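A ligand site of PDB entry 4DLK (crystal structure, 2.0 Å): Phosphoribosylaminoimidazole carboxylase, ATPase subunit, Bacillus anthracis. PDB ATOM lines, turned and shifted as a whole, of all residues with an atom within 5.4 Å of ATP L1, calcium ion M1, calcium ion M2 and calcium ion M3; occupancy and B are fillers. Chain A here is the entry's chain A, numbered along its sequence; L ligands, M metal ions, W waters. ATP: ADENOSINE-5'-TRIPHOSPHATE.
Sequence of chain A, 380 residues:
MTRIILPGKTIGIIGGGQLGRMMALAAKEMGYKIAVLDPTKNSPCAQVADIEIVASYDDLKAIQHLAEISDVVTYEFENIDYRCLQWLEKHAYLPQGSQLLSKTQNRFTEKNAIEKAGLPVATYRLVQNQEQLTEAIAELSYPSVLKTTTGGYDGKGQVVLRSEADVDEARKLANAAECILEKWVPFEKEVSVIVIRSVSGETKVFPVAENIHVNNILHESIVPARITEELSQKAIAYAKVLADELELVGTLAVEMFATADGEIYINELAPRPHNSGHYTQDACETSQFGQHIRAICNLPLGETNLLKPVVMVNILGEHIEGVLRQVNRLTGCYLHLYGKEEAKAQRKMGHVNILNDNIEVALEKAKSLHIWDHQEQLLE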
ATOM      1  N   ARG A 107      25.480  27.218  24.172  1.00  0.00           N
ATOM      2  CA  ARG A 107      24.308  26.623  23.491  1.00  0.00           C
ATOM      3  C   ARG A 107      23.031  27.457  23.695  1.00  0.00           C
ATOM      4  O   ARG A 107      22.229  27.573  22.777  1.00  0.00           O
ATOM      5  CB  ARG A 107      24.058  25.187  23.969  1.00  0.00           C
ATOM      6  CG  ARG A 107      25.130  24.165  23.614  1.00  0.00           C
ATOM      7  CD  ARG A 107      24.602  22.749  23.862  1.00  0.00           C
ATOM      8  NE  ARG A 107      25.629  21.714  23.737  1.00  0.00           N
ATOM      9  CZ  ARG A 107      26.132  21.290  22.580  1.00  0.00           C
ATOM     10  NH1 ARG A 107      27.061  20.331  22.579  1.00  0.00           N
ATOM     11  NH2 ARG A 107      25.730  21.802  21.424  1.00  0.00           N
ATOM     12  N   ALA A 122      14.793  23.408  18.119  1.00  0.00           N
ATOM     13  CA  ALA A 122      14.030  22.621  19.078  1.00  0.00           C
ATOM     14  C   ALA A 122      13.638  23.507  20.263  1.00  0.00           C
ATOM     15  O   ALA A 122      14.437  24.345  20.693  1.00  0.00           O
ATOM     16  CB  ALA A 122      14.837  21.425  19.552  1.00  0.00           C
ATOM     17  N   VAL A 145      16.459  16.197  25.798  1.00  0.00           N
ATOM     18  CA  VAL A 145      17.905  16.067  25.931  1.00  0.00           C
ATOM     19  C   VAL A 145      18.506  17.240  26.711  1.00  0.00           C
ATOM     20  O   VAL A 145      18.291  18.421  26.379  1.00  0.00           O
ATOM     21  CB  VAL A 145      18.583  15.871  24.539  1.00  0.00           C
ATOM     22  CG1 VAL A 145      18.344  17.062  23.631  1.00  0.00           C
ATOM     23  CG2 VAL A 145      20.069  15.597  24.683  1.00  0.00           C
ATOM     24  N   LYS A 147      21.792  19.238  27.770  1.00  0.00           N
ATOM     25  CA  LYS A 147      23.168  19.498  27.331  1.00  0.00           C
ATOM     26  C   LYS A 147      23.799  20.617  28.144  1.00  0.00           C
ATOM     27  O   LYS A 147      23.136  21.614  28.437  1.00  0.00           O
ATOM     28  CB  LYS A 147      23.206  19.941  25.873  1.00  0.00           C
ATOM     29  CG  LYS A 147      22.444  19.072  24.893  1.00  0.00           C
ATOM     30  CD  LYS A 147      22.471  19.688  23.509  1.00  0.00           C
ATOM     31  CE  LYS A 147      21.543  18.944  22.561  1.00  0.00           C
ATOM     32  NZ  LYS A 147      21.637  19.480  21.178  1.00  0.00           N
ATOM     33  N   GLY A 152      30.744  21.348  25.820  1.00  0.00           N
ATOM     34  CA  GLY A 152      30.203  20.092  25.318  1.00  0.00           C
ATOM     35  C   GLY A 152      30.726  19.768  23.928  1.00  0.00           C
ATOM     36  O   GLY A 152      30.774  20.630  23.050  1.00  0.00           O
ATOM     37  N   TYR A 153      31.120  18.514  23.719  1.00  0.00           N
ATOM     38  CA  TYR A 153      31.621  18.065  22.413  1.00  0.00           C
ATOM     39  C   TYR A 153      31.555  16.543  22.361  1.00  0.00           C
ATOM     40  O   TYR A 153      31.526  15.885  23.396  1.00  0.00           O
ATOM     41  CB  TYR A 153      33.060  18.554  22.184  1.00  0.00           C
ATOM     42  CG  TYR A 153      34.107  17.895  23.061  1.00  0.00           C
ATOM     43  CD1 TYR A 153      34.910  16.868  22.566  1.00  0.00           C
ATOM     44  CD2 TYR A 153      34.286  18.297  24.387  1.00  0.00           C
ATOM     45  CE1 TYR A 153      35.866  16.261  23.365  1.00  0.00           C
ATOM     46  CE2 TYR A 153      35.241  17.684  25.199  1.00  0.00           C
ATOM     47  CZ  TYR A 153      36.017  16.669  24.684  1.00  0.00           C
ATOM     48  OH  TYR A 153      36.968  16.053  25.463  1.00  0.00           O
ATOM     49  N   ASP A 154      31.526  16.006  21.143  1.00  0.00           N
ATOM     50  CA  ASP A 154      31.473  14.551  20.935  1.00  0.00           C
ATOM     51  C   ASP A 154      30.423  13.898  21.835  1.00  0.00           C
ATOM     52  O   ASP A 154      30.677  12.855  22.436  1.00  0.00           O
ATOM     53  CB  ASP A 154      32.860  13.922  21.174  1.00  0.00           C
ATOM     54  CG  ASP A 154      33.878  14.292  20.097  1.00  0.00           C
ATOM     55  OD1 ASP A 154      35.048  13.902  20.236  1.00  0.00           O
ATOM     56  OD2 ASP A 154      33.516  14.957  19.102  1.00  0.00           O
ATOM     57  N   GLY A 155      29.261  14.533  21.963  1.00  0.00           N
ATOM     58  CA  GLY A 155      28.173  13.994  22.793  1.00  0.00           C
ATOM     59  C   GLY A 155      28.430  13.963  24.288  1.00  0.00           C
ATOM     60  O   GLY A 155      27.615  13.447  25.042  1.00  0.00           O
ATOM     61  N   LYS A 156      29.566  14.516  24.725  1.00  0.00           N
ATOM     62  CA  LYS A 156      29.900  14.581  26.152  1.00  0.00           C
ATOM     63  C   LYS A 156      29.154  15.724  26.801  1.00  0.00           C
ATOM     64  O   LYS A 156      28.948  16.770  26.182  1.00  0.00           O
ATOM     65  CB  LYS A 156      31.398  14.785  26.362  1.00  0.00           C
ATOM     66  CG  LYS A 156      32.293  13.666  25.843  1.00  0.00           C
ATOM     67  CD  LYS A 156      33.751  14.090  25.974  1.00  0.00           C
ATOM     68  CE  LYS A 156      34.660  13.222  25.116  1.00  0.00           C
ATOM     69  NZ  LYS A 156      34.660  11.812  25.603  1.00  0.00           N
ATOM     70  N   GLN A 158      26.029  15.355  27.967  1.00  0.00           N
ATOM     71  CA  GLN A 158      24.722  15.193  27.352  1.00  0.00           C
ATOM     72  C   GLN A 158      24.003  13.999  27.956  1.00  0.00           C
ATOM     73  O   GLN A 158      24.570  12.915  28.096  1.00  0.00           O
ATOM     74  CB  GLN A 158      24.876  15.019  25.833  1.00  0.00           C
ATOM     75  CG  GLN A 158      23.665  15.429  25.022  1.00  0.00           C
ATOM     76  CD  GLN A 158      24.017  15.761  23.582  1.00  0.00           C
ATOM     77  OE1 GLN A 158      24.724  16.738  23.301  1.00  0.00           O
ATOM     78  NE2 GLN A 158      23.507  14.953  22.664  1.00  0.00           N
ATOM     79  N   GLU A 182      16.432  20.452  25.781  1.00  0.00           N
ATOM     80  CA  GLU A 182      15.825  20.561  24.460  1.00  0.00           C
ATOM     81  C   GLU A 182      14.839  19.446  24.266  1.00  0.00           C
ATOM     82  O   GLU A 182      15.085  18.324  24.679  1.00  0.00           O
ATOM     83  CB  GLU A 182      16.884  20.421  23.370  1.00  0.00           C
ATOM     84  CG  GLU A 182      17.817  21.599  23.177  1.00  0.00           C
ATOM     85  CD  GLU A 182      18.821  21.345  22.073  1.00  0.00           C
ATOM     86  OE1 GLU A 182      19.822  22.081  22.021  1.00  0.00           O
ATOM     87  OE2 GLU A 182      18.601  20.402  21.260  1.00  0.00           O
ATOM     88  N   LYS A 183      13.729  19.735  23.604  1.00  0.00           N
ATOM     89  CA  LYS A 183      12.809  18.708  23.161  1.00  0.00           C
ATOM     90  C   LYS A 183      13.497  17.829  22.134  1.00  0.00           C
ATOM     91  O   LYS A 183      14.249  18.322  21.280  1.00  0.00           O
ATOM     92  CB  LYS A 183      11.539  19.340  22.578  1.00  0.00           C
ATOM     93  CG  LYS A 183      10.389  18.361  22.391  1.00  0.00           C
ATOM     94  CD  LYS A 183       9.083  19.098  22.127  1.00  0.00           C
ATOM     95  CE  LYS A 183       7.909  18.122  22.131  1.00  0.00           C
ATOM     96  NZ  LYS A 183       6.607  18.836  22.220  1.00  0.00           N
ATOM     97  N   TRP A 184      13.272  16.524  22.230  1.00  0.00           N
ATOM     98  CA  TRP A 184      13.820  15.580  21.272  1.00  0.00           C
ATOM     99  C   TRP A 184      13.165  15.790  19.936  1.00  0.00           C
ATOM    100  O   TRP A 184      11.928  15.830  19.836  1.00  0.00           O
ATOM    101  CB  TRP A 184      13.600  14.151  21.755  1.00  0.00           C
ATOM    102  CG  TRP A 184      14.164  13.098  20.844  1.00  0.00           C
ATOM    103  CD1 TRP A 184      13.511  12.437  19.800  1.00  0.00           C
ATOM    104  CD2 TRP A 184      15.522  12.543  20.859  1.00  0.00           C
ATOM    105  NE1 TRP A 184      14.356  11.536  19.186  1.00  0.00           N
ATOM    106  CE2 TRP A 184      15.579  11.555  19.772  1.00  0.00           C
ATOM    107  CE3 TRP A 184      16.660  12.772  21.620  1.00  0.00           C
ATOM    108  CZ2 TRP A 184      16.719  10.825  19.501  1.00  0.00           C
ATOM    109  CZ3 TRP A 184      17.812  12.032  21.330  1.00  0.00           C
ATOM    110  CH2 TRP A 184      17.843  11.081  20.303  1.00  0.00           C
ATOM    111  N   VAL A 185      13.976  15.952  18.900  1.00  0.00           N
ATOM    112  CA  VAL A 185      13.472  16.138  17.543  1.00  0.00           C
ATOM    113  C   VAL A 185      13.530  14.784  16.855  1.00  0.00           C
ATOM    114  O   VAL A 185      14.623  14.232  16.679  1.00  0.00           O
ATOM    115  CB  VAL A 185      14.331  17.160  16.738  1.00  0.00           C
ATOM    116  CG1 VAL A 185      13.778  17.342  15.329  1.00  0.00           C
ATOM    117  CG2 VAL A 185      14.386  18.506  17.462  1.00  0.00           C
ATOM    118  N   PRO A 186      12.371  14.212  16.493  1.00  0.00           N
ATOM    119  CA  PRO A 186      12.405  13.026  15.652  1.00  0.00           C
ATOM    120  C   PRO A 186      12.725  13.430  14.201  1.00  0.00           C
ATOM    121  O   PRO A 186      11.876  13.966  13.496  1.00  0.00           O
ATOM    122  CB  PRO A 186      10.982  12.459  15.772  1.00  0.00           C
ATOM    123  CG  PRO A 186      10.124  13.628  16.122  1.00  0.00           C
ATOM    124  CD  PRO A 186      10.995  14.619  16.847  1.00  0.00           C
ATOM    125  N   PHE A 187      13.968  13.220  13.782  1.00  0.00           N
ATOM    126  CA  PHE A 187      14.374  13.612  12.433  1.00  0.00           C
ATOM    127  C   PHE A 187      14.744  12.374  11.635  1.00  0.00           C
ATOM    128  O   PHE A 187      14.988  11.312  12.198  1.00  0.00           O
ATOM    129  CB  PHE A 187      15.557  14.592  12.470  1.00  0.00           C
ATOM    130  CG  PHE A 187      16.750  14.062  13.220  1.00  0.00           C
ATOM    131  CD1 PHE A 187      16.931  14.380  14.565  1.00  0.00           C
ATOM    132  CD2 PHE A 187      17.697  13.255  12.592  1.00  0.00           C
ATOM    133  CE1 PHE A 187      18.025  13.897  15.267  1.00  0.00           C
ATOM    134  CE2 PHE A 187      18.780  12.765  13.290  1.00  0.00           C
ATOM    135  CZ  PHE A 187      18.955  13.082  14.626  1.00  0.00           C
ATOM    136  N   GLU A 190      20.453  14.066   9.572  1.00  0.00           N
ATOM    137  CA  GLU A 190      21.207  15.239   9.987  1.00  0.00           C
ATOM    138  C   GLU A 190      21.932  15.776   8.780  1.00  0.00           C
ATOM    139  O   GLU A 190      22.575  15.004   8.042  1.00  0.00           O
ATOM    140  CB  GLU A 190      22.209  14.894  11.086  1.00  0.00           C
ATOM    141  CG  GLU A 190      21.579  14.245  12.292  1.00  0.00           C
ATOM    142  CD  GLU A 190      22.521  14.162  13.475  1.00  0.00           C
ATOM    143  OE1 GLU A 190      22.751  13.041  13.957  1.00  0.00           O
ATOM    144  OE2 GLU A 190      23.026  15.225  13.900  1.00  0.00           O
ATOM    145  N   HIS A 213      26.953  10.207  11.777  1.00  0.00           N
ATOM    146  CA  HIS A 213      27.845  10.136  12.930  1.00  0.00           C
ATOM    147  C   HIS A 213      27.786   8.757  13.533  1.00  0.00           C
ATOM    148  O   HIS A 213      26.714   8.138  13.582  1.00  0.00           O
ATOM    149  CB  HIS A 213      27.492  11.190  13.982  1.00  0.00           C
ATOM    150  CG  HIS A 213      27.495  12.608  13.445  1.00  0.00           C
ATOM    151  ND1 HIS A 213      26.452  13.128  12.780  1.00  0.00           N
ATOM    152  CD2 HIS A 213      28.470  13.599  13.493  1.00  0.00           C
ATOM    153  CE1 HIS A 213      26.746  14.399  12.420  1.00  0.00           C
ATOM    154  NE2 HIS A 213      27.988  14.683  12.851  1.00  0.00           N
ATOM    155  N   ASN A 216      29.441   9.305  18.202  1.00  0.00           N
ATOM    156  CA  ASN A 216      29.612  10.749  18.362  1.00  0.00           C
ATOM    157  C   ASN A 216      30.812  11.351  17.622  1.00  0.00           C
ATOM    158  O   ASN A 216      31.368  12.362  18.044  1.00  0.00           O
ATOM    159  CB  ASN A 216      29.608  11.155  19.836  1.00  0.00           C
ATOM    160  CG  ASN A 216      28.215  11.094  20.444  1.00  0.00           C
ATOM    161  OD1 ASN A 216      27.345  11.904  20.116  1.00  0.00           O
ATOM    162  ND2 ASN A 216      28.007  10.134  21.336  1.00  0.00           N
ATOM    163  N   GLU A 255      24.616  23.215  11.128  1.00  0.00           N
ATOM    164  CA  GLU A 255      24.176  21.825  11.271  1.00  0.00           C
ATOM    165  C   GLU A 255      22.692  21.780  11.615  1.00  0.00           C
ATOM    166  O   GLU A 255      22.211  22.556  12.454  1.00  0.00           O
ATOM    167  CB  GLU A 255      25.025  21.079  12.303  1.00  0.00           C
ATOM    168  CG  GLU A 255      26.495  20.963  11.911  1.00  0.00           C
ATOM    169  CD  GLU A 255      27.325  20.257  12.974  1.00  0.00           C
ATOM    170  OE1 GLU A 255      27.983  20.940  13.789  1.00  0.00           O
ATOM    171  OE2 GLU A 255      27.321  19.007  13.011  1.00  0.00           O
ATOM    172  N   PHE A 257      18.680  19.426  11.617  1.00  0.00           N
ATOM    173  CA  PHE A 257      17.881  18.226  11.611  1.00  0.00           C
ATOM    174  C   PHE A 257      16.813  18.362  10.525  1.00  0.00           C
ATOM    175  O   PHE A 257      16.166  19.411  10.425  1.00  0.00           O
ATOM    176  CB  PHE A 257      17.175  18.004  12.953  1.00  0.00           C
ATOM    177  CG  PHE A 257      18.093  17.901  14.141  1.00  0.00           C
ATOM    178  CD1 PHE A 257      17.780  18.556  15.335  1.00  0.00           C
ATOM    179  CD2 PHE A 257      19.263  17.139  14.090  1.00  0.00           C
ATOM    180  CE1 PHE A 257      18.616  18.447  16.444  1.00  0.00           C
ATOM    181  CE2 PHE A 257      20.101  17.050  15.184  1.00  0.00           C
ATOM    182  CZ  PHE A 257      19.771  17.698  16.366  1.00  0.00           C
ATOM    183  N   ASN A 267      20.440  22.974  14.536  1.00  0.00           N
ATOM    184  CA  ASN A 267      20.968  22.279  15.702  1.00  0.00           C
ATOM    185  C   ASN A 267      22.085  23.060  16.365  1.00  0.00           C
ATOM    186  O   ASN A 267      21.973  23.447  17.531  1.00  0.00           O
ATOM    187  CB  ASN A 267      21.439  20.865  15.308  1.00  0.00           C
ATOM    188  CG  ASN A 267      22.070  20.115  16.474  1.00  0.00           C
ATOM    189  OD1 ASN A 267      21.649  20.251  17.630  1.00  0.00           O
ATOM    190  ND2 ASN A 267      23.076  19.301  16.164  1.00  0.00           N
ATOM    191  N   GLU A 268      23.173  23.281  15.624  1.00  0.00           N
ATOM    192  CA  GLU A 268      24.248  24.155  16.092  1.00  0.00           C
ATOM    193  C   GLU A 268      25.025  24.820  14.959  1.00  0.00           C
ATOM    194  O   GLU A 268      24.867  24.479  13.792  1.00  0.00           O
ATOM    195  CB  GLU A 268      25.188  23.428  17.077  1.00  0.00           C
ATOM    196  CG  GLU A 268      25.608  22.026  16.654  1.00  0.00           C
ATOM    197  CD  GLU A 268      26.680  21.440  17.556  1.00  0.00           C
ATOM    198  OE1 GLU A 268      26.699  21.722  18.780  1.00  0.00           O
ATOM    199  OE2 GLU A 268      27.521  20.675  17.060  1.00  0.00           O
ATOM    200  N   HIS A 274      34.505  23.340   8.703  1.00  0.00           N
ATOM    201  CA  HIS A 274      33.923  22.246   9.484  1.00  0.00           C
ATOM    202  C   HIS A 274      34.179  20.935   8.800  1.00  0.00           C
ATOM    203  O   HIS A 274      34.312  20.882   7.578  1.00  0.00           O
ATOM    204  CB  HIS A 274      32.425  22.509   9.596  1.00  0.00           C
ATOM    205  CG  HIS A 274      31.710  21.583  10.538  1.00  0.00           C
ATOM    206  ND1 HIS A 274      31.041  20.499  10.122  1.00  0.00           N
ATOM    207  CD2 HIS A 274      31.565  21.628  11.933  1.00  0.00           C
ATOM    208  CE1 HIS A 274      30.513  19.850  11.182  1.00  0.00           C
ATOM    209  NE2 HIS A 274      30.821  20.555  12.293  1.00  0.00           N
ATOM    210  N   LYS A 348      41.190  12.211  14.601  1.00  0.00           N
ATOM    211  CA  LYS A 348      41.032  12.372  13.162  1.00  0.00           C
ATOM    212  C   LYS A 348      42.387  12.562  12.483  1.00  0.00           C
ATOM    213  O   LYS A 348      43.061  13.565  12.703  1.00  0.00           O
ATOM    214  CB  LYS A 348      40.098  13.549  12.839  1.00  0.00           C
ATOM    215  CG  LYS A 348      38.652  13.268  13.194  1.00  0.00           C
ATOM    216  CD  LYS A 348      37.755  14.510  13.125  1.00  0.00           C
ATOM    217  CE  LYS A 348      36.405  14.209  13.764  1.00  0.00           C
ATOM    218  NZ  LYS A 348      35.453  15.351  13.679  1.00  0.00           N
HETATM  219  PG  ATP L   1      29.776  17.094  18.125  1.00  0.00           P
HETATM  220  O1G ATP L   1      29.203  18.377  17.568  1.00  0.00           O
HETATM  221  O2G ATP L   1      29.614  15.918  17.179  1.00  0.00           O
HETATM  222  O3G ATP L   1      31.167  17.245  18.689  1.00  0.00           O
HETATM  223  PB  ATP L   1      27.856  17.613  20.231  1.00  0.00           P
HETATM  224  O1B ATP L   1      27.453  16.834  21.438  1.00  0.00           O
HETATM  225  O2B ATP L   1      28.360  19.024  20.341  1.00  0.00           O
HETATM  226  O3B ATP L   1      28.932  16.689  19.440  1.00  0.00           O
HETATM  227  PA  ATP L   1      25.115  17.845  19.357  1.00  0.00           P
HETATM  228  O1A ATP L   1      24.551  18.119  17.993  1.00  0.00           O
HETATM  229  O2A ATP L   1      24.906  18.842  20.466  1.00  0.00           O
HETATM  230  O3A ATP L   1      26.678  17.567  19.136  1.00  0.00           O
HETATM  231  O5' ATP L   1      24.508  16.431  19.830  1.00  0.00           O
HETATM  232  C5' ATP L   1      25.034  15.206  19.313  1.00  0.00           C
HETATM  233  C4' ATP L   1      23.931  14.327  18.733  1.00  0.00           C
HETATM  234  O4' ATP L   1      22.840  14.206  19.655  1.00  0.00           O
HETATM  235  C3' ATP L   1      23.331  14.905  17.457  1.00  0.00           C
HETATM  236  O3' ATP L   1      24.044  14.485  16.289  1.00  0.00           O
HETATM  237  C2' ATP L   1      21.905  14.375  17.469  1.00  0.00           C
HETATM  238  O2' ATP L   1      21.847  13.103  16.822  1.00  0.00           O
HETATM  239  C1' ATP L   1      21.602  14.173  18.938  1.00  0.00           C
HETATM  240  N9  ATP L   1      20.725  15.273  19.365  1.00  0.00           N
HETATM  241  C8  ATP L   1      21.130  16.424  19.950  1.00  0.00           C
HETATM  242  N7  ATP L   1      20.068  17.227  20.213  1.00  0.00           N
HETATM  243  C5  ATP L   1      18.963  16.597  19.800  1.00  0.00           C
HETATM  244  C6  ATP L   1      17.509  16.885  19.788  1.00  0.00           C
HETATM  245  N6  ATP L   1      17.034  18.049  20.291  1.00  0.00           N
HETATM  246  N1  ATP L   1      16.685  15.951  19.253  1.00  0.00           N
HETATM  247  C2  ATP L   1      17.148  14.788  18.757  1.00  0.00           C
HETATM  248  N3  ATP L   1      18.457  14.453  18.745  1.00  0.00           N
HETATM  249  C4  ATP L   1      19.397  15.307  19.240  1.00  0.00           C
HETATM  250  PG  ATP L   2      31.498  17.735  14.215  1.00  0.00           P
HETATM  251  O1G ATP L   2      32.295  17.453  15.471  1.00  0.00           O
HETATM  252  O2G ATP L   2      31.061  16.507  13.456  1.00  0.00           O
HETATM  253  O3G ATP L   2      30.398  18.764  14.386  1.00  0.00           O
HETATM  254  PB  ATP L   2      33.745  19.384  13.661  1.00  0.00           P
HETATM  255  O1B ATP L   2      34.292  20.159  12.471  1.00  0.00           O
HETATM  256  O2B ATP L   2      33.261  20.149  14.880  1.00  0.00           O
HETATM  257  O3B ATP L   2      32.552  18.414  13.181  1.00  0.00           O
HETATM  258  PA  ATP L   2      36.447  18.511  13.935  1.00  0.00           P
HETATM  259  O1A ATP L   2      36.808  18.548  12.470  1.00  0.00           O
HETATM  260  O2A ATP L   2      37.091  17.497  14.859  1.00  0.00           O
HETATM  261  O3A ATP L   2      34.852  18.318  14.138  1.00  0.00           O
HETATM  262  O5' ATP L   2      36.682  19.971  14.538  1.00  0.00           O
HETATM  263  C5' ATP L   2      37.997  20.484  14.702  1.00  0.00           C
HETATM  264  C4' ATP L   2      37.803  21.684  15.606  1.00  0.00           C
HETATM  265  O4' ATP L   2      37.355  21.258  16.891  1.00  0.00           O
HETATM  266  C3' ATP L   2      39.085  22.473  15.800  1.00  0.00           C
HETATM  267  O3' ATP L   2      38.730  23.845  15.585  1.00  0.00           O
HETATM  268  C2' ATP L   2      39.465  22.225  17.252  1.00  0.00           C
HETATM  269  O2' ATP L   2      40.103  23.371  17.824  1.00  0.00           O
HETATM  270  C1' ATP L   2      38.093  21.960  17.890  1.00  0.00           C
HETATM  271  N9  ATP L   2      38.154  21.191  19.163  1.00  0.00           N
HETATM  272  C8  ATP L   2      39.013  20.203  19.491  1.00  0.00           C
HETATM  273  N7  ATP L   2      38.774  19.737  20.745  1.00  0.00           N
HETATM  274  C5  ATP L   2      37.727  20.425  21.245  1.00  0.00           C
HETATM  275  C6  ATP L   2      36.965  20.438  22.506  1.00  0.00           C
HETATM  276  N6  ATP L   2      37.279  19.590  23.512  1.00  0.00           N
HETATM  277  N1  ATP L   2      35.938  21.316  22.634  1.00  0.00           N
HETATM  278  C2  ATP L   2      35.612  22.180  21.633  1.00  0.00           C
HETATM  279  N3  ATP L   2      36.272  22.217  20.455  1.00  0.00           N
HETATM  280  C4  ATP L   2      37.321  21.387  20.203  1.00  0.00           C
HETATM  281 CA    CA M   1      29.108  20.514  18.771  1.00  0.00          CA
HETATM  282 CA    CA M   2      28.316  19.073  15.457  1.00  0.00          CA
HETATM  283 CA    CA M   3      33.209  16.756  17.531  1.00  0.00          CA
HETATM  284  O   HOH W   1      27.885  16.612  15.105  1.00  0.00           O
HETATM  285  O   HOH W   2      23.397  20.919  19.600  1.00  0.00           O
HETATM  286  O   HOH W   3      27.670  17.647  23.953  1.00  0.00           O
HETATM  287  O   HOH W   4      34.889  17.996  19.006  1.00  0.00           O
HETATM  288  O   HOH W   5      34.464  19.919  17.601  1.00  0.00           O
HETATM  289  O   HOH W   6      29.263  21.770  20.799  1.00  0.00           O
HETATM  290  O   HOH W   7      29.846  22.655  18.102  1.00  0.00           O
HETATM  291  O   HOH W   8      28.167  13.773  17.804  1.00  0.00           O
HETATM  292  O   HOH W   9      35.331  16.420  16.544  1.00  0.00           O
HETATM  293  O   HOH W  10      31.884  14.844  16.808  1.00  0.00           O
HETATM  294  O   HOH W  11      19.158  11.844  17.684  1.00  0.00           O
HETATM  295  O   HOH W  12      25.904  18.419  15.689  1.00  0.00           O
HETATM  296  O   HOH W  13      30.220  21.132  15.997  1.00  0.00           O
HETATM  297  O   HOH W  14      31.313  19.942  19.171  1.00  0.00           O
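Calcium ion M1 is bound by O2B of ATP L1 (2.3 Å). Water W14 is bound to calcium ion M1, 2.3 Å away. Calcium ion M1 is bound by the side-chain carboxylate (OE2) of Glu 268 (2.3 Å). Water W7 is bound to calcium ion M1 (2.4 Å). Calcium ion M1 is bound by water W6, 2.4 Å away. O1G of ATP L1 is bound to calcium ion M1, at 2.5 Å. OE1 of Glu 268 binds calcium ion M1 (2.7 Å). Slightly farther from calcium ion M1 lies water W13 (3.1 Å).
O3B of ATP L1 sits at hydrogen-bond distance from N of Asp 154, 3.2 Å away. An oxygen (O1A) of ATP L1 is in hydrogen-bond range of the side-chain amide nitrogen (ND2) of Asn 267 (2.6 Å). The side-chain carboxylate (OE2) of Glu 190 sits at hydrogen-bond distance from an oxygen (O3') of ATP L1 (2.7 Å). The backbone NH (N) of Val 185 sits at hydrogen-bond distance from a nitrogen (N1) of ATP L1 (2.7 Å). An oxygen (O2A) of ATP L1 is in salt-bridge range of the guanidinium group (NH2) of Arg 107 (3.2 Å). NZ of Lys 147 lies within salt-bridge range of O2A of ATP L1 (3.4 Å). O of Lys 183 lies within hydrogen-bond range of N6 of ATP L1. The backbone NH of Gly 155 sits at hydrogen-bond distance from an oxygen (O1B) of ATP L1 (3.0 Å). The side-chain carboxylate of Glu 182 is in hydrogen-bond range of a nitrogen (N6) of ATP L1 (3.0 Å). O4' of ATP L1 is in hydrogen-bond range of NE2 of Gln 158 (3.2 Å). An oxygen (O3B) of ATP L2 is in hydrogen-bond range of a ring nitrogen (NE2) of His 274 (2.9 Å). The side-chain amino group (NZ) of Lys 348 lies within salt-bridge range of an oxygen (O2A) of ATP L2 (2.9 Å).
One residue has an atom within 4 Å of calcium ion M3: Asp 154.
Calcium ion M2 is bound by O3G of ATP L2, O1G of ATP L1, OE2 of Glu 268, water W12, water W1, OE1 of Glu 255, OE2 of Glu 255 and water W13. Calcium ion M2 has eight donor atoms within binding distance.
Merely in contact with ATP L1: Val 145 (3.7 Å), Gly 152 (3.97 Å), Tyr 153 (3.8 Å), Trp 184 (3.5 Å), Phe 187 (3.5 Å) and Phe 257 (3.7 Å). Hydrophobic or aromatic side chains within 4 Å of ATP L1: Val 145, Trp 184, Val 185, Phe 187 and Phe 257. The nearest printed residue that does not touch ATP L1 is Asn 216 (4.1 Å).
The guanidinium group of Arg 107 lies close to the side-chain carboxylate of Glu 268, 2.8 Å away. O of Glu 255 is in hydrogen-bond range of N of Asn 267, at 2.8 Å. The side-chain carboxylate (OE1) of Glu 255 sits close to a ring nitrogen (NE2) of His 274, 3.2 Å away. The side-chain carboxylate of Glu 182 lies within salt-bridge range of the side-chain amino group of Lys 147. O of Glu 182 sits at hydrogen-bond distance from N of Val 145 (2.8 Å).
Within 4 Å of calcium ion M2: Glu 255 and Glu 268. The nearest printed residue that does not touch calcium ion M2 is His 274 (4.3 Å).
Water W6 bridges O of Gly 152 (2.9 Å) and NH1 of Arg 107 (3.2 Å). Water W12 bridges an oxygen (O1A) of ATP L1 (2.7 Å) and the side-chain amide nitrogen (ND2) of Asn 267 (3.0 Å). Water W10 bridges O2G of ATP L1 (2.5 Å) and O of Asn 216 (2.8 Å). Water W9 bridges an oxygen (O2A) of ATP L2 (2.7 Å) and the side-chain amino group of Lys 348 (3.1 Å). Water W3 lies within hydrogen-bond range of an oxygen (O1B) of ATP L1, the backbone carbonyl oxygen (O) of Lys 156, the guanidinium group (NH1) of Arg 107 and the side-chain amide oxygen (OE1) of Gln 158. Water W8 bridges O2G of ATP L1 and OD1 of Asn 216.
Calcium ion M3 is bound by O1G of ATP L2, water W9, O3G of ATP L1, OD2 of Asp 154, water W10 and water W4. Calcium ion M3 has six donor atoms within binding distance.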
